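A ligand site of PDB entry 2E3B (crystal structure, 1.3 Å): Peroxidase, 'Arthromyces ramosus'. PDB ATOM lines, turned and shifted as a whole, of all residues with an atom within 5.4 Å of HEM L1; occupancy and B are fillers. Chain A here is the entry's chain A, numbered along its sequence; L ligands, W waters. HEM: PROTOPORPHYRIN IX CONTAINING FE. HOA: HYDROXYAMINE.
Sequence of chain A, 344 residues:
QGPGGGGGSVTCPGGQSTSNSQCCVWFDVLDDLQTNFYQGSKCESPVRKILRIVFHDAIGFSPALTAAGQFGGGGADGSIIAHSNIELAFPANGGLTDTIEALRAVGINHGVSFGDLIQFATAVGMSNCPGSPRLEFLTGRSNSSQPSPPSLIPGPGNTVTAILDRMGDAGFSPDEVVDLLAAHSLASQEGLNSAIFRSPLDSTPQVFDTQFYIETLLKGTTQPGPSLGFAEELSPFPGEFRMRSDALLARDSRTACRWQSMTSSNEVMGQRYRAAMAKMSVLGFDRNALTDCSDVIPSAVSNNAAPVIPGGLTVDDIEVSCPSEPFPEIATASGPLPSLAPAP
An oxygen (O1A) of HEM L1 lies within hydrogen-bond range of the backbone NH (N) of Glu 190 (2.8 Å). OG of Ser 188 lies within hydrogen-bond range of O2D of HEM L1. The backbone NH (N) of Ser 188 is in hydrogen-bond range of an oxygen (O2D) of HEM L1 (2.8 Å). The guanidinium group (NH1) of Arg 52 is in salt-bridge range of an oxygen (O1A) of HEM L1, 3.9 Å away. NE of Arg 48 lies within salt-bridge range of O2D of HEM L1 (2.8 Å). The backbone NH of Gly 191 is in hydrogen-bond range of an oxygen (O2A) of HEM L1, at 2.8 Å. An iron atom (FE) of HEM L1 is bound by a ring nitrogen (NE2) of His 184 (2.0 Å).
FE of HEM L1 is bound by N of HOA L2 (2.1 Å).
N of Ser 245 is in hydrogen-bond range of O of Pro 156, at 2.9 Å. The backbone carbonyl oxygen of Ala 187 is in hydrogen-bond range of the backbone NH of Leu 201, at 2.8 Å. OE1 of Glu 190 lies within salt-bridge range of NZ of Lys 49 (2.8 Å). The side-chain sulfur (SD) of Met 243 lies close to the side-chain hydroxyl (OG) of Ser 245 (3.4 Å). N of Leu 192 is in hydrogen-bond range of OE1 of Gln 189 (2.8 Å). N of Gly 191 lies within hydrogen-bond range of OE1 of Gln 189 (3.3 Å).
Merely in contact with HEM L1: Phe 55, Leu 186, Met 243, Ala 183, Leu 51, Ala 187, Leu 181, Gly 155, Ser 245, Leu 192, Pro 156, Gln 189, Leu 180, Pro 154, Met 277 and Lys 49. Hydrophobic or aromatic side chains within 4 Å of HEM L1: Leu 51, Phe 55, Pro 154, Pro 156, Leu 180, Leu 181, Ala 183, His 184, Ala 187, Leu 192, Met 243 and Met 277. 22 residues have an atom within 4 Å of HEM L1: Arg 48, Lys 49, Leu 51, Arg 52, Phe 55, Pro 154, Gly 155, Pro 156, Leu 180, Leu 181, Ala 183, His 184, Leu 186, Ala 187, Ser 188, Gln 189, Glu 190, Gly 191, Leu 192, Met 243, Ser 245 and Met 277.
Water W6 lies within hydrogen-bond range of an oxygen (O1D) of HEM L1 (2.7 Å), the side-chain hydroxyl (OG) of Ser 45 (2.7 Å), the side-chain carboxylate (OE2) of Glu 190 (2.7 Å) and the guanidinium group (NH1) of Arg 48 (2.9 Å). Water W5 lies within hydrogen-bond range of an oxygen (O1D) of HEM L1 (2.7 Å), the side-chain amino group (NZ) of Lys 49 (2.8 Å) and the guanidinium group (NH1) of Arg 52 (2.8 Å). Water W2 lies within hydrogen-bond range of an oxygen (O1A) of HEM L1 (2.8 Å) and the guanidinium group (NH1) of Arg 52 (3.1 Å).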
ATOM      1  N   SER A  45      10.492 -29.284  18.377  1.00  0.00           N
ATOM      2  CA  SER A  45       9.091 -28.997  18.391  1.00  0.00           C
ATOM      3  C   SER A  45       8.542 -28.806  19.803  1.00  0.00           C
ATOM      4  O   SER A  45       7.759 -27.861  19.964  1.00  0.00           O
ATOM      5  CB  SER A  45       8.340 -30.085  17.638  1.00  0.00           C
ATOM      6  OG  SER A  45       6.980 -29.735  17.588  1.00  0.00           O
ATOM      7  N   VAL A  47       9.684 -27.340  22.468  1.00  0.00           N
ATOM      8  CA  VAL A  47       9.825 -25.971  22.937  1.00  0.00           C
ATOM      9  C   VAL A  47       8.920 -25.047  22.151  1.00  0.00           C
ATOM     10  O   VAL A  47       8.321 -24.117  22.697  1.00  0.00           O
ATOM     11  CB  VAL A  47      11.283 -25.450  22.853  1.00  0.00           C
ATOM     12  CG1 VAL A  47      11.340 -24.095  23.565  1.00  0.00           C
ATOM     13  CG2 VAL A  47      12.299 -26.368  23.461  1.00  0.00           C
ATOM     14  N   ARG A  48       8.864 -25.275  20.852  1.00  0.00           N
ATOM     15  CA  ARG A  48       8.064 -24.373  20.012  1.00  0.00           C
ATOM     16  C   ARG A  48       6.589 -24.455  20.341  1.00  0.00           C
ATOM     17  O   ARG A  48       5.924 -23.424  20.407  1.00  0.00           O
ATOM     18  CB  ARG A  48       8.318 -24.670  18.535  1.00  0.00           C
ATOM     19  CG  ARG A  48       9.811 -24.688  18.194  1.00  0.00           C
ATOM     20  CD  ARG A  48      10.062 -24.611  16.688  1.00  0.00           C
ATOM     21  NE  ARG A  48       9.479 -25.759  16.019  1.00  0.00           N
ATOM     22  CZ  ARG A  48      10.069 -26.906  15.705  1.00  0.00           C
ATOM     23  NH1 ARG A  48       9.379 -27.848  15.102  1.00  0.00           N
ATOM     24  NH2 ARG A  48      11.348 -27.092  15.999  1.00  0.00           N
ATOM     25  N   LYS A  49       6.135 -25.664  20.582  1.00  0.00           N
ATOM     26  CA  LYS A  49       4.746 -25.812  21.038  1.00  0.00           C
ATOM     27  C   LYS A  49       4.542 -25.155  22.401  1.00  0.00           C
ATOM     28  O   LYS A  49       3.505 -24.540  22.623  1.00  0.00           O
ATOM     29  CB  LYS A  49       4.377 -27.280  21.142  1.00  0.00           C
ATOM     30  CG  LYS A  49       4.398 -28.011  19.793  1.00  0.00           C
ATOM     31  CD  LYS A  49       3.247 -27.646  18.921  1.00  0.00           C
ATOM     32  CE  LYS A  49       3.313 -28.448  17.636  1.00  0.00           C
ATOM     33  NZ  LYS A  49       2.127 -28.153  16.784  1.00  0.00           N
ATOM     34  N   LEU A  51       6.058 -22.603  23.525  1.00  0.00           N
ATOM     35  CA  LEU A  51       5.983 -21.139  23.373  1.00  0.00           C
ATOM     36  C   LEU A  51       4.615 -20.728  22.878  1.00  0.00           C
ATOM     37  O   LEU A  51       4.093 -19.706  23.270  1.00  0.00           O
ATOM     38  CB  LEU A  51       7.122 -20.710  22.477  1.00  0.00           C
ATOM     39  CG  LEU A  51       8.505 -20.765  23.115  1.00  0.00           C
ATOM     40  CD1 LEU A  51       9.553 -20.559  22.077  1.00  0.00           C
ATOM     41  CD2 LEU A  51       8.594 -19.714  24.216  1.00  0.00           C
ATOM     42  N   ARG A  52       4.008 -21.448  21.963  1.00  0.00           N
ATOM     43  CA  ARG A  52       2.628 -21.137  21.622  1.00  0.00           C
ATOM     44  C   ARG A  52       1.741 -21.247  22.846  1.00  0.00           C
ATOM     45  O   ARG A  52       0.875 -20.405  23.063  1.00  0.00           O
ATOM     46  CB  ARG A  52       2.127 -22.097  20.550  1.00  0.00           C
ATOM     47  CG  ARG A  52       2.657 -21.788  19.176  1.00  0.00           C
ATOM     48  CD  ARG A  52       2.121 -22.705  18.092  1.00  0.00           C
ATOM     49  NE  ARG A  52       0.671 -22.590  17.976  1.00  0.00           N
ATOM     50  CZ  ARG A  52      -0.161 -23.569  17.652  1.00  0.00           C
ATOM     51  NH1 ARG A  52       0.271 -24.786  17.375  1.00  0.00           N
ATOM     52  NH2 ARG A  52      -1.463 -23.291  17.603  1.00  0.00           N
ATOM     53  N   VAL A  54       2.511 -20.882  26.034  1.00  0.00           N
ATOM     54  CA  VAL A  54       2.680 -19.886  27.083  1.00  0.00           C
ATOM     55  C   VAL A  54       1.979 -18.617  26.703  1.00  0.00           C
ATOM     56  O   VAL A  54       1.350 -17.952  27.468  1.00  0.00           O
ATOM     57  CB  VAL A  54       4.167 -19.707  27.442  1.00  0.00           C
ATOM     58  CG1 VAL A  54       4.931 -19.025  26.316  1.00  0.00           C
ATOM     59  CG2 VAL A  54       4.322 -18.920  28.735  1.00  0.00           C
ATOM     60  N   PHE A  55       2.099 -18.259  25.425  1.00  0.00           N
ATOM     61  CA  PHE A  55       1.417 -17.097  24.918  1.00  0.00           C
ATOM     62  C   PHE A  55      -0.081 -17.288  24.978  1.00  0.00           C
ATOM     63  O   PHE A  55      -0.814 -16.410  25.441  1.00  0.00           O
ATOM     64  CB  PHE A  55       1.907 -16.858  23.494  1.00  0.00           C
ATOM     65  CG  PHE A  55       1.240 -15.738  22.744  1.00  0.00           C
ATOM     66  CD1 PHE A  55       0.865 -14.552  23.372  1.00  0.00           C
ATOM     67  CD2 PHE A  55       0.963 -15.865  21.397  1.00  0.00           C
ATOM     68  CE1 PHE A  55       0.246 -13.568  22.666  1.00  0.00           C
ATOM     69  CE2 PHE A  55       0.328 -14.868  20.678  1.00  0.00           C
ATOM     70  CZ  PHE A  55      -0.019 -13.684  21.317  1.00  0.00           C
ATOM     71  N   PRO A 154      -4.520 -13.332  19.264  1.00  0.00           N
ATOM     72  CA  PRO A 154      -4.267 -12.775  17.934  1.00  0.00           C
ATOM     73  C   PRO A 154      -4.067 -13.880  16.911  1.00  0.00           C
ATOM     74  O   PRO A 154      -3.404 -14.871  17.195  1.00  0.00           O
ATOM     75  CB  PRO A 154      -2.990 -11.959  18.129  1.00  0.00           C
ATOM     76  CG  PRO A 154      -3.009 -11.589  19.567  1.00  0.00           C
ATOM     77  CD  PRO A 154      -3.605 -12.744  20.274  1.00  0.00           C
ATOM     78  N   GLY A 155      -4.629 -13.701  15.726  1.00  0.00           N
ATOM     79  CA  GLY A 155      -4.487 -14.669  14.655  1.00  0.00           C
ATOM     80  C   GLY A 155      -3.716 -14.061  13.497  1.00  0.00           C
ATOM     81  O   GLY A 155      -3.553 -12.856  13.371  1.00  0.00           O
ATOM     82  N   PRO A 156      -3.171 -14.954  12.682  1.00  0.00           N
ATOM     83  CA  PRO A 156      -2.235 -14.542  11.641  1.00  0.00           C
ATOM     84  C   PRO A 156      -2.863 -13.770  10.492  1.00  0.00           C
ATOM     85  O   PRO A 156      -2.142 -13.132   9.751  1.00  0.00           O
ATOM     86  CB  PRO A 156      -1.672 -15.863  11.137  1.00  0.00           C
ATOM     87  CG  PRO A 156      -2.757 -16.846  11.418  1.00  0.00           C
ATOM     88  CD  PRO A 156      -3.306 -16.399  12.742  1.00  0.00           C
ATOM     89  N   ILE A 163      -4.265  -6.688  16.049  1.00  0.00           N
ATOM     90  CA  ILE A 163      -3.261  -7.321  16.889  1.00  0.00           C
ATOM     91  C   ILE A 163      -2.816  -6.381  17.988  1.00  0.00           C
ATOM     92  O   ILE A 163      -2.767  -6.745  19.131  1.00  0.00           O
ATOM     93  CB  ILE A 163      -2.061  -7.782  16.073  1.00  0.00           C
ATOM     94  CG1 ILE A 163      -2.535  -8.858  15.077  1.00  0.00           C
ATOM     95  CG2 ILE A 163      -0.921  -8.244  16.955  1.00  0.00           C
ATOM     96  CD1 ILE A 163      -1.423  -9.275  14.138  1.00  0.00           C
ATOM     97  N   MET A 167      -3.379  -7.059  21.865  1.00  0.00           N
ATOM     98  CA  MET A 167      -2.193  -7.161  22.700  1.00  0.00           C
ATOM     99  C   MET A 167      -2.165  -5.973  23.651  1.00  0.00           C
ATOM    100  O   MET A 167      -1.768  -6.123  24.824  1.00  0.00           O
ATOM    101  CB  MET A 167      -0.937  -7.163  21.861  1.00  0.00           C
ATOM    102  CG  MET A 167      -0.766  -8.392  21.001  1.00  0.00           C
ATOM    103  SD  MET A 167      -0.606  -9.917  21.956  1.00  0.00           S
ATOM    104  CE  MET A 167       1.133  -9.853  22.416  1.00  0.00           C
ATOM    105  N   VAL A 177       4.951  -6.060  21.655  1.00  0.00           N
ATOM    106  CA  VAL A 177       4.446  -7.054  20.728  1.00  0.00           C
ATOM    107  C   VAL A 177       5.600  -7.543  19.862  1.00  0.00           C
ATOM    108  O   VAL A 177       5.779  -8.720  19.663  1.00  0.00           O
ATOM    109  CB  VAL A 177       3.277  -6.519  19.880  1.00  0.00           C
ATOM    110  CG1 VAL A 177       2.943  -7.509  18.788  1.00  0.00           C
ATOM    111  CG2 VAL A 177       2.090  -6.214  20.797  1.00  0.00           C
ATOM    112  N   LEU A 180       7.970  -9.675  21.932  1.00  0.00           N
ATOM    113  CA  LEU A 180       7.475 -11.007  22.197  1.00  0.00           C
ATOM    114  C   LEU A 180       7.610 -11.906  20.965  1.00  0.00           C
ATOM    115  O   LEU A 180       7.793 -13.116  21.084  1.00  0.00           O
ATOM    116  CB  LEU A 180       6.012 -10.957  22.606  1.00  0.00           C
ATOM    117  CG  LEU A 180       5.729 -10.467  24.030  1.00  0.00           C
ATOM    118  CD1 LEU A 180       4.236 -10.257  24.185  1.00  0.00           C
ATOM    119  CD2 LEU A 180       6.274 -11.420  25.077  1.00  0.00           C
ATOM    120  N   LEU A 181       7.494 -11.296  19.794  1.00  0.00           N
ATOM    121  CA  LEU A 181       7.576 -12.060  18.561  1.00  0.00           C
ATOM    122  C   LEU A 181       8.973 -12.542  18.292  1.00  0.00           C
ATOM    123  O   LEU A 181       9.136 -13.327  17.344  1.00  0.00           O
ATOM    124  CB  LEU A 181       7.047 -11.237  17.390  1.00  0.00           C
ATOM    125  CG  LEU A 181       5.544 -11.396  17.244  1.00  0.00           C
ATOM    126  CD1 LEU A 181       4.979 -10.263  16.427  1.00  0.00           C
ATOM    127  CD2 LEU A 181       5.198 -12.738  16.587  1.00  0.00           C
ATOM    128  N   ALA A 183      10.004 -14.908  19.719  1.00  0.00           N
ATOM    129  CA  ALA A 183       9.768 -16.332  19.767  1.00  0.00           C
ATOM    130  C   ALA A 183       9.595 -16.909  18.366  1.00  0.00           C
ATOM    131  O   ALA A 183       9.856 -18.096  18.175  1.00  0.00           O
ATOM    132  CB  ALA A 183       8.539 -16.656  20.581  1.00  0.00           C
ATOM    133  N   HIS A 184       9.218 -16.135  17.377  1.00  0.00           N
ATOM    134  CA  HIS A 184       9.136 -16.652  16.031  1.00  0.00           C
ATOM    135  C   HIS A 184      10.507 -16.890  15.434  1.00  0.00           C
ATOM    136  O   HIS A 184      10.588 -17.422  14.331  1.00  0.00           O
ATOM    137  CB  HIS A 184       8.274 -15.765  15.127  1.00  0.00           C
ATOM    138  CG  HIS A 184       6.812 -15.979  15.340  1.00  0.00           C
ATOM    139  ND1 HIS A 184       5.856 -15.477  14.490  1.00  0.00           N
ATOM    140  CD2 HIS A 184       6.128 -16.615  16.323  1.00  0.00           C
ATOM    141  CE1 HIS A 184       4.667 -15.816  14.944  1.00  0.00           C
ATOM    142  NE2 HIS A 184       4.776 -16.524  16.059  1.00  0.00           N
ATOM    143  N   LEU A 186      12.165 -19.154  16.812  1.00  0.00           N
ATOM    144  CA  LEU A 186      12.255 -20.564  17.133  1.00  0.00           C
ATOM    145  C   LEU A 186      10.952 -21.177  16.711  1.00  0.00           C
ATOM    146  O   LEU A 186      10.173 -21.641  17.529  1.00  0.00           O
ATOM    147  CB  LEU A 186      12.397 -20.749  18.630  1.00  0.00           C
ATOM    148  CG  LEU A 186      13.692 -20.220  19.225  1.00  0.00           C
ATOM    149  CD1 LEU A 186      13.571 -20.339  20.747  1.00  0.00           C
ATOM    150  CD2 LEU A 186      14.912 -20.962  18.722  1.00  0.00           C
ATOM    151  N   ALA A 187      10.680 -21.180  15.406  1.00  0.00           N
ATOM    152  CA  ALA A 187       9.313 -21.366  15.014  1.00  0.00           C
ATOM    153  C   ALA A 187       9.153 -21.988  13.625  1.00  0.00           C
ATOM    154  O   ALA A 187       9.938 -21.826  12.703  1.00  0.00           O
ATOM    155  CB  ALA A 187       8.583 -20.013  14.976  1.00  0.00           C
ATOM    156  N   SER A 188       8.046 -22.696  13.512  1.00  0.00           N
ATOM    157  CA  SER A 188       7.532 -23.236  12.253  1.00  0.00           C
ATOM    158  C   SER A 188       6.017 -23.133  12.275  1.00  0.00           C
ATOM    159  O   SER A 188       5.425 -22.758  13.278  1.00  0.00           O
ATOM    160  CB  SER A 188       8.015 -24.659  12.078  1.00  0.00           C
ATOM    161  OG  SER A 188       7.279 -25.581  12.858  1.00  0.00           O
ATOM    162  N   GLN A 189       5.406 -23.521  11.160  1.00  0.00           N
ATOM    163  CA  GLN A 189       3.980 -23.790  11.212  1.00  0.00           C
ATOM    164  C   GLN A 189       3.738 -25.245  10.877  1.00  0.00           C
ATOM    165  O   GLN A 189       4.428 -25.764   9.982  1.00  0.00           O
ATOM    166  CB  GLN A 189       3.242 -22.856  10.273  1.00  0.00           C
ATOM    167  CG  GLN A 189       3.528 -22.988   8.772  1.00  0.00           C
ATOM    168  CD  GLN A 189       2.779 -24.129   8.059  1.00  0.00           C
ATOM    169  OE1 GLN A 189       1.656 -24.441   8.571  1.00  0.00           O
ATOM    170  NE2 GLN A 189       3.392 -24.772   7.115  1.00  0.00           N
ATOM    171  N   GLU A 190       2.684 -25.772  11.417  1.00  0.00           N
ATOM    172  CA  GLU A 190       2.159 -27.049  11.045  1.00  0.00           C
ATOM    173  C   GLU A 190       0.711 -26.965  10.582  1.00  0.00           C
ATOM    174  O   GLU A 190       0.274 -27.862   9.861  1.00  0.00           O
ATOM    175  CB  GLU A 190       2.154 -27.995  12.241  1.00  0.00           C
ATOM    176  CG  GLU A 190       3.552 -28.329  12.728  1.00  0.00           C
ATOM    177  CD  GLU A 190       3.574 -29.168  13.957  1.00  0.00           C
ATOM    178  OE1 GLU A 190       2.500 -29.593  14.431  1.00  0.00           O
ATOM    179  OE2 GLU A 190       4.704 -29.395  14.436  1.00  0.00           O
ATOM    180  N   GLY A 191      -0.050 -25.962  11.006  1.00  0.00           N
ATOM    181  CA  GLY A 191      -1.463 -25.951  10.827  1.00  0.00           C
ATOM    182  C   GLY A 191      -1.937 -24.992   9.766  1.00  0.00           C
ATOM    183  O   GLY A 191      -3.101 -25.028   9.460  1.00  0.00           O
ATOM    184  N   LEU A 192      -1.070 -24.132   9.245  1.00  0.00           N
ATOM    185  CA  LEU A 192      -1.468 -23.175   8.238  1.00  0.00           C
ATOM    186  C   LEU A 192      -1.385 -23.744   6.842  1.00  0.00           C
ATOM    187  O   LEU A 192      -2.232 -23.460   6.000  1.00  0.00           O
ATOM    188  CB  LEU A 192      -0.606 -21.902   8.318  1.00  0.00           C
ATOM    189  CG  LEU A 192      -0.716 -21.175   9.674  1.00  0.00           C
ATOM    190  CD1 LEU A 192       0.215 -19.993   9.753  1.00  0.00           C
ATOM    191  CD2 LEU A 192      -2.138 -20.675   9.984  1.00  0.00           C
ATOM    192  N   LEU A 201       9.806 -20.365  10.264  1.00  0.00           N
ATOM    193  CA  LEU A 201       9.583 -18.933  10.098  1.00  0.00           C
ATOM    194  C   LEU A 201      10.872 -18.168   9.944  1.00  0.00           C
ATOM    195  O   LEU A 201      10.824 -17.038   9.483  1.00  0.00           O
ATOM    196  CB  LEU A 201       8.752 -18.385  11.227  1.00  0.00           C
ATOM    197  CG  LEU A 201       7.478 -19.112  11.602  1.00  0.00           C
ATOM    198  CD1 LEU A 201       6.693 -18.321  12.658  1.00  0.00           C
ATOM    199  CD2 LEU A 201       6.594 -19.316  10.366  1.00  0.00           C
ATOM    200  N   MET A 243       3.927 -15.779   7.618  1.00  0.00           N
ATOM    201  CA  MET A 243       2.517 -15.559   7.923  1.00  0.00           C
ATOM    202  C   MET A 243       2.264 -14.078   7.760  1.00  0.00           C
ATOM    203  O   MET A 243       3.144 -13.221   7.907  1.00  0.00           O
ATOM    204  CB  MET A 243       2.102 -16.052   9.297  1.00  0.00           C
ATOM    205  CG  MET A 243       2.539 -15.193  10.457  1.00  0.00           C
ATOM    206  SD  MET A 243       2.138 -15.952  12.022  1.00  0.00           S
ATOM    207  CE  MET A 243       3.301 -17.327  12.016  1.00  0.00           C
ATOM    208  N   SER A 245       0.491 -11.842   9.445  1.00  0.00           N
ATOM    209  CA  SER A 245       0.670 -10.928  10.562  1.00  0.00           C
ATOM    210  C   SER A 245       2.144 -10.534  10.692  1.00  0.00           C
ATOM    211  O   SER A 245       2.382  -9.340  10.954  1.00  0.00           O
ATOM    212  CB  SER A 245       0.151 -11.566  11.814  1.00  0.00           C
ATOM    213  OG  SER A 245       0.671 -12.843  11.993  1.00  0.00           O
ATOM    214  N   LEU A 249       3.490  -6.771  10.375  1.00  0.00           N
ATOM    215  CA  LEU A 249       4.092  -6.129  11.511  1.00  0.00           C
ATOM    216  C   LEU A 249       5.490  -5.640  11.212  1.00  0.00           C
ATOM    217  O   LEU A 249       5.922  -4.599  11.696  1.00  0.00           O
ATOM    218  CB  LEU A 249       4.088  -7.122  12.691  1.00  0.00           C
ATOM    219  CG  LEU A 249       2.769  -7.364  13.393  1.00  0.00           C
ATOM    220  CD1 LEU A 249       2.737  -8.611  14.234  1.00  0.00           C
ATOM    221  CD2 LEU A 249       2.469  -6.140  14.255  1.00  0.00           C
ATOM    222  N   TYR A 273      13.116  -9.498  24.843  1.00  0.00           N
ATOM    223  CA  TYR A 273      12.248 -10.668  24.939  1.00  0.00           C
ATOM    224  C   TYR A 273      12.100 -11.119  26.380  1.00  0.00           C
ATOM    225  O   TYR A 273      11.004 -11.398  26.857  1.00  0.00           O
ATOM    226  CB  TYR A 273      12.818 -11.745  24.077  1.00  0.00           C
ATOM    227  CG  TYR A 273      12.092 -13.042  24.056  1.00  0.00           C
ATOM    228  CD1 TYR A 273      10.908 -13.209  23.385  1.00  0.00           C
ATOM    229  CD2 TYR A 273      12.637 -14.128  24.711  1.00  0.00           C
ATOM    230  CE1 TYR A 273      10.255 -14.416  23.388  1.00  0.00           C
ATOM    231  CE2 TYR A 273      12.007 -15.352  24.707  1.00  0.00           C
ATOM    232  CZ  TYR A 273      10.804 -15.499  24.034  1.00  0.00           C
ATOM    233  OH  TYR A 273      10.155 -16.716  23.969  1.00  0.00           O
ATOM    234  N   MET A 277       8.553 -11.266  28.150  1.00  0.00           N
ATOM    235  CA  MET A 277       8.081 -12.553  28.618  1.00  0.00           C
ATOM    236  C   MET A 277       7.828 -12.516  30.125  1.00  0.00           C
ATOM    237  O   MET A 277       6.863 -13.120  30.586  1.00  0.00           O
ATOM    238  CB  MET A 277       9.096 -13.640  28.328  1.00  0.00           C
ATOM    239  CG  MET A 277       9.231 -13.982  26.845  1.00  0.00           C
ATOM    240  SD  MET A 277       7.694 -14.675  26.177  1.00  0.00           S
ATOM    241  CE  MET A 277       7.896 -16.382  26.732  1.00  0.00           C
ATOM    242  N   MET A 280       4.534 -10.936  30.463  1.00  0.00           N
ATOM    243  CA  MET A 280       3.441 -11.806  30.057  1.00  0.00           C
ATOM    244  C   MET A 280       3.220 -12.888  31.087  1.00  0.00           C
ATOM    245  O   MET A 280       2.091 -13.364  31.274  1.00  0.00           O
ATOM    246  CB  MET A 280       3.819 -12.437  28.694  1.00  0.00           C
ATOM    247  CG  MET A 280       2.678 -13.244  28.175  1.00  0.00           C
ATOM    248  SD  MET A 280       2.884 -13.682  26.431  1.00  0.00           S
ATOM    249  CE  MET A 280       3.981 -15.063  26.678  1.00  0.00           C
HETATM  250  CHA HEM L   1       3.789 -20.237  15.559  1.00  0.00           C
HETATM  251  CHB HEM L   1       0.708 -16.628  15.052  1.00  0.00           C
HETATM  252  CHC HEM L   1       2.895 -14.350  18.626  1.00  0.00           C
HETATM  253  CHD HEM L   1       5.399 -18.302  19.644  1.00  0.00           C
HETATM  254  C1A HEM L   1       2.758 -19.479  15.097  1.00  0.00           C
HETATM  255  C2A HEM L   1       1.754 -19.932  14.150  1.00  0.00           C
HETATM  256  C3A HEM L   1       0.869 -18.926  14.029  1.00  0.00           C
HETATM  257  C4A HEM L   1       1.275 -17.870  14.946  1.00  0.00           C
HETATM  258  CMA HEM L   1      -0.364 -18.843  13.146  1.00  0.00           C
HETATM  259  CAA HEM L   1       1.818 -21.234  13.414  1.00  0.00           C
HETATM  260  CBA HEM L   1       1.239 -22.342  14.279  1.00  0.00           C
HETATM  261  CGA HEM L   1       1.067 -23.600  13.438  1.00  0.00           C
HETATM  262  O1A HEM L   1       1.653 -24.650  13.772  1.00  0.00           O
HETATM  263  O2A HEM L   1       0.385 -23.534  12.404  1.00  0.00           O
HETATM  264  C1B HEM L   1       1.103 -15.625  15.903  1.00  0.00           C
HETATM  265  C2B HEM L   1       0.515 -14.318  15.964  1.00  0.00           C
HETATM  266  C3B HEM L   1       1.169 -13.618  16.948  1.00  0.00           C
HETATM  267  C4B HEM L   1       2.141 -14.551  17.500  1.00  0.00           C
HETATM  268  CMB HEM L   1      -0.625 -13.856  15.082  1.00  0.00           C
HETATM  269  CAB HEM L   1       0.866 -12.265  17.310  1.00  0.00           C
HETATM  270  CBB HEM L   1       1.737 -11.303  17.836  1.00  0.00           C
HETATM  271  C1C HEM L   1       3.657 -15.250  19.315  1.00  0.00           C
HETATM  272  C2C HEM L   1       4.220 -15.079  20.624  1.00  0.00           C
HETATM  273  C3C HEM L   1       4.894 -16.222  20.931  1.00  0.00           C
HETATM  274  C4C HEM L   1       4.742 -17.094  19.782  1.00  0.00           C
HETATM  275  CMC HEM L   1       4.054 -13.829  21.448  1.00  0.00           C
HETATM  276  CAC HEM L   1       5.493 -16.677  22.134  1.00  0.00           C
HETATM  277  CBC HEM L   1       6.255 -15.786  22.987  1.00  0.00           C
HETATM  278  C1D HEM L   1       5.285 -19.117  18.518  1.00  0.00           C
HETATM  279  C2D HEM L   1       6.102 -20.273  18.226  1.00  0.00           C
HETATM  280  C3D HEM L   1       5.660 -20.804  17.089  1.00  0.00           C
HETATM  281  C4D HEM L   1       4.582 -19.991  16.648  1.00  0.00           C
HETATM  282  CMD HEM L   1       7.299 -20.695  19.053  1.00  0.00           C
HETATM  283  CAD HEM L   1       6.204 -22.029  16.405  1.00  0.00           C
HETATM  284  CBD HEM L   1       5.400 -23.289  16.735  1.00  0.00           C
HETATM  285  CGD HEM L   1       5.970 -24.535  16.089  1.00  0.00           C
HETATM  286  O1D HEM L   1       5.323 -25.567  16.308  1.00  0.00           O
HETATM  287  O2D HEM L   1       7.061 -24.462  15.499  1.00  0.00           O
HETATM  288  NA  HEM L   1       2.396 -18.246  15.644  1.00  0.00           N
HETATM  289  NB  HEM L   1       2.077 -15.772  16.861  1.00  0.00           N
HETATM  290  NC  HEM L   1       3.950 -16.505  18.801  1.00  0.00           N
HETATM  291  ND  HEM L   1       4.378 -18.950  17.502  1.00  0.00           N
HETATM  292 FE   HEM L   1       3.288 -17.327  17.144  1.00  0.00          FE
HETATM  293  N   HOA L   2       1.652 -18.016  18.217  1.00  0.00           N
HETATM  294  O   HOA L   2       2.063 -18.524  19.506  1.00  0.00           O
HETATM  295  O   HOH W   1       2.407 -12.457  13.983  1.00  0.00           O
HETATM  296  O   HOH W   2      -0.344 -26.393  14.791  1.00  0.00           O
HETATM  297  O   HOH W   3      -2.185 -16.964  16.702  1.00  0.00           O
HETATM  298  O   HOH W   4      -2.166 -22.682  12.927  1.00  0.00           O
HETATM  299  O   HOH W   5       2.663 -25.526  16.113  1.00  0.00           O
HETATM  300  O   HOH W   6       6.557 -27.840  15.686  1.00  0.00           O
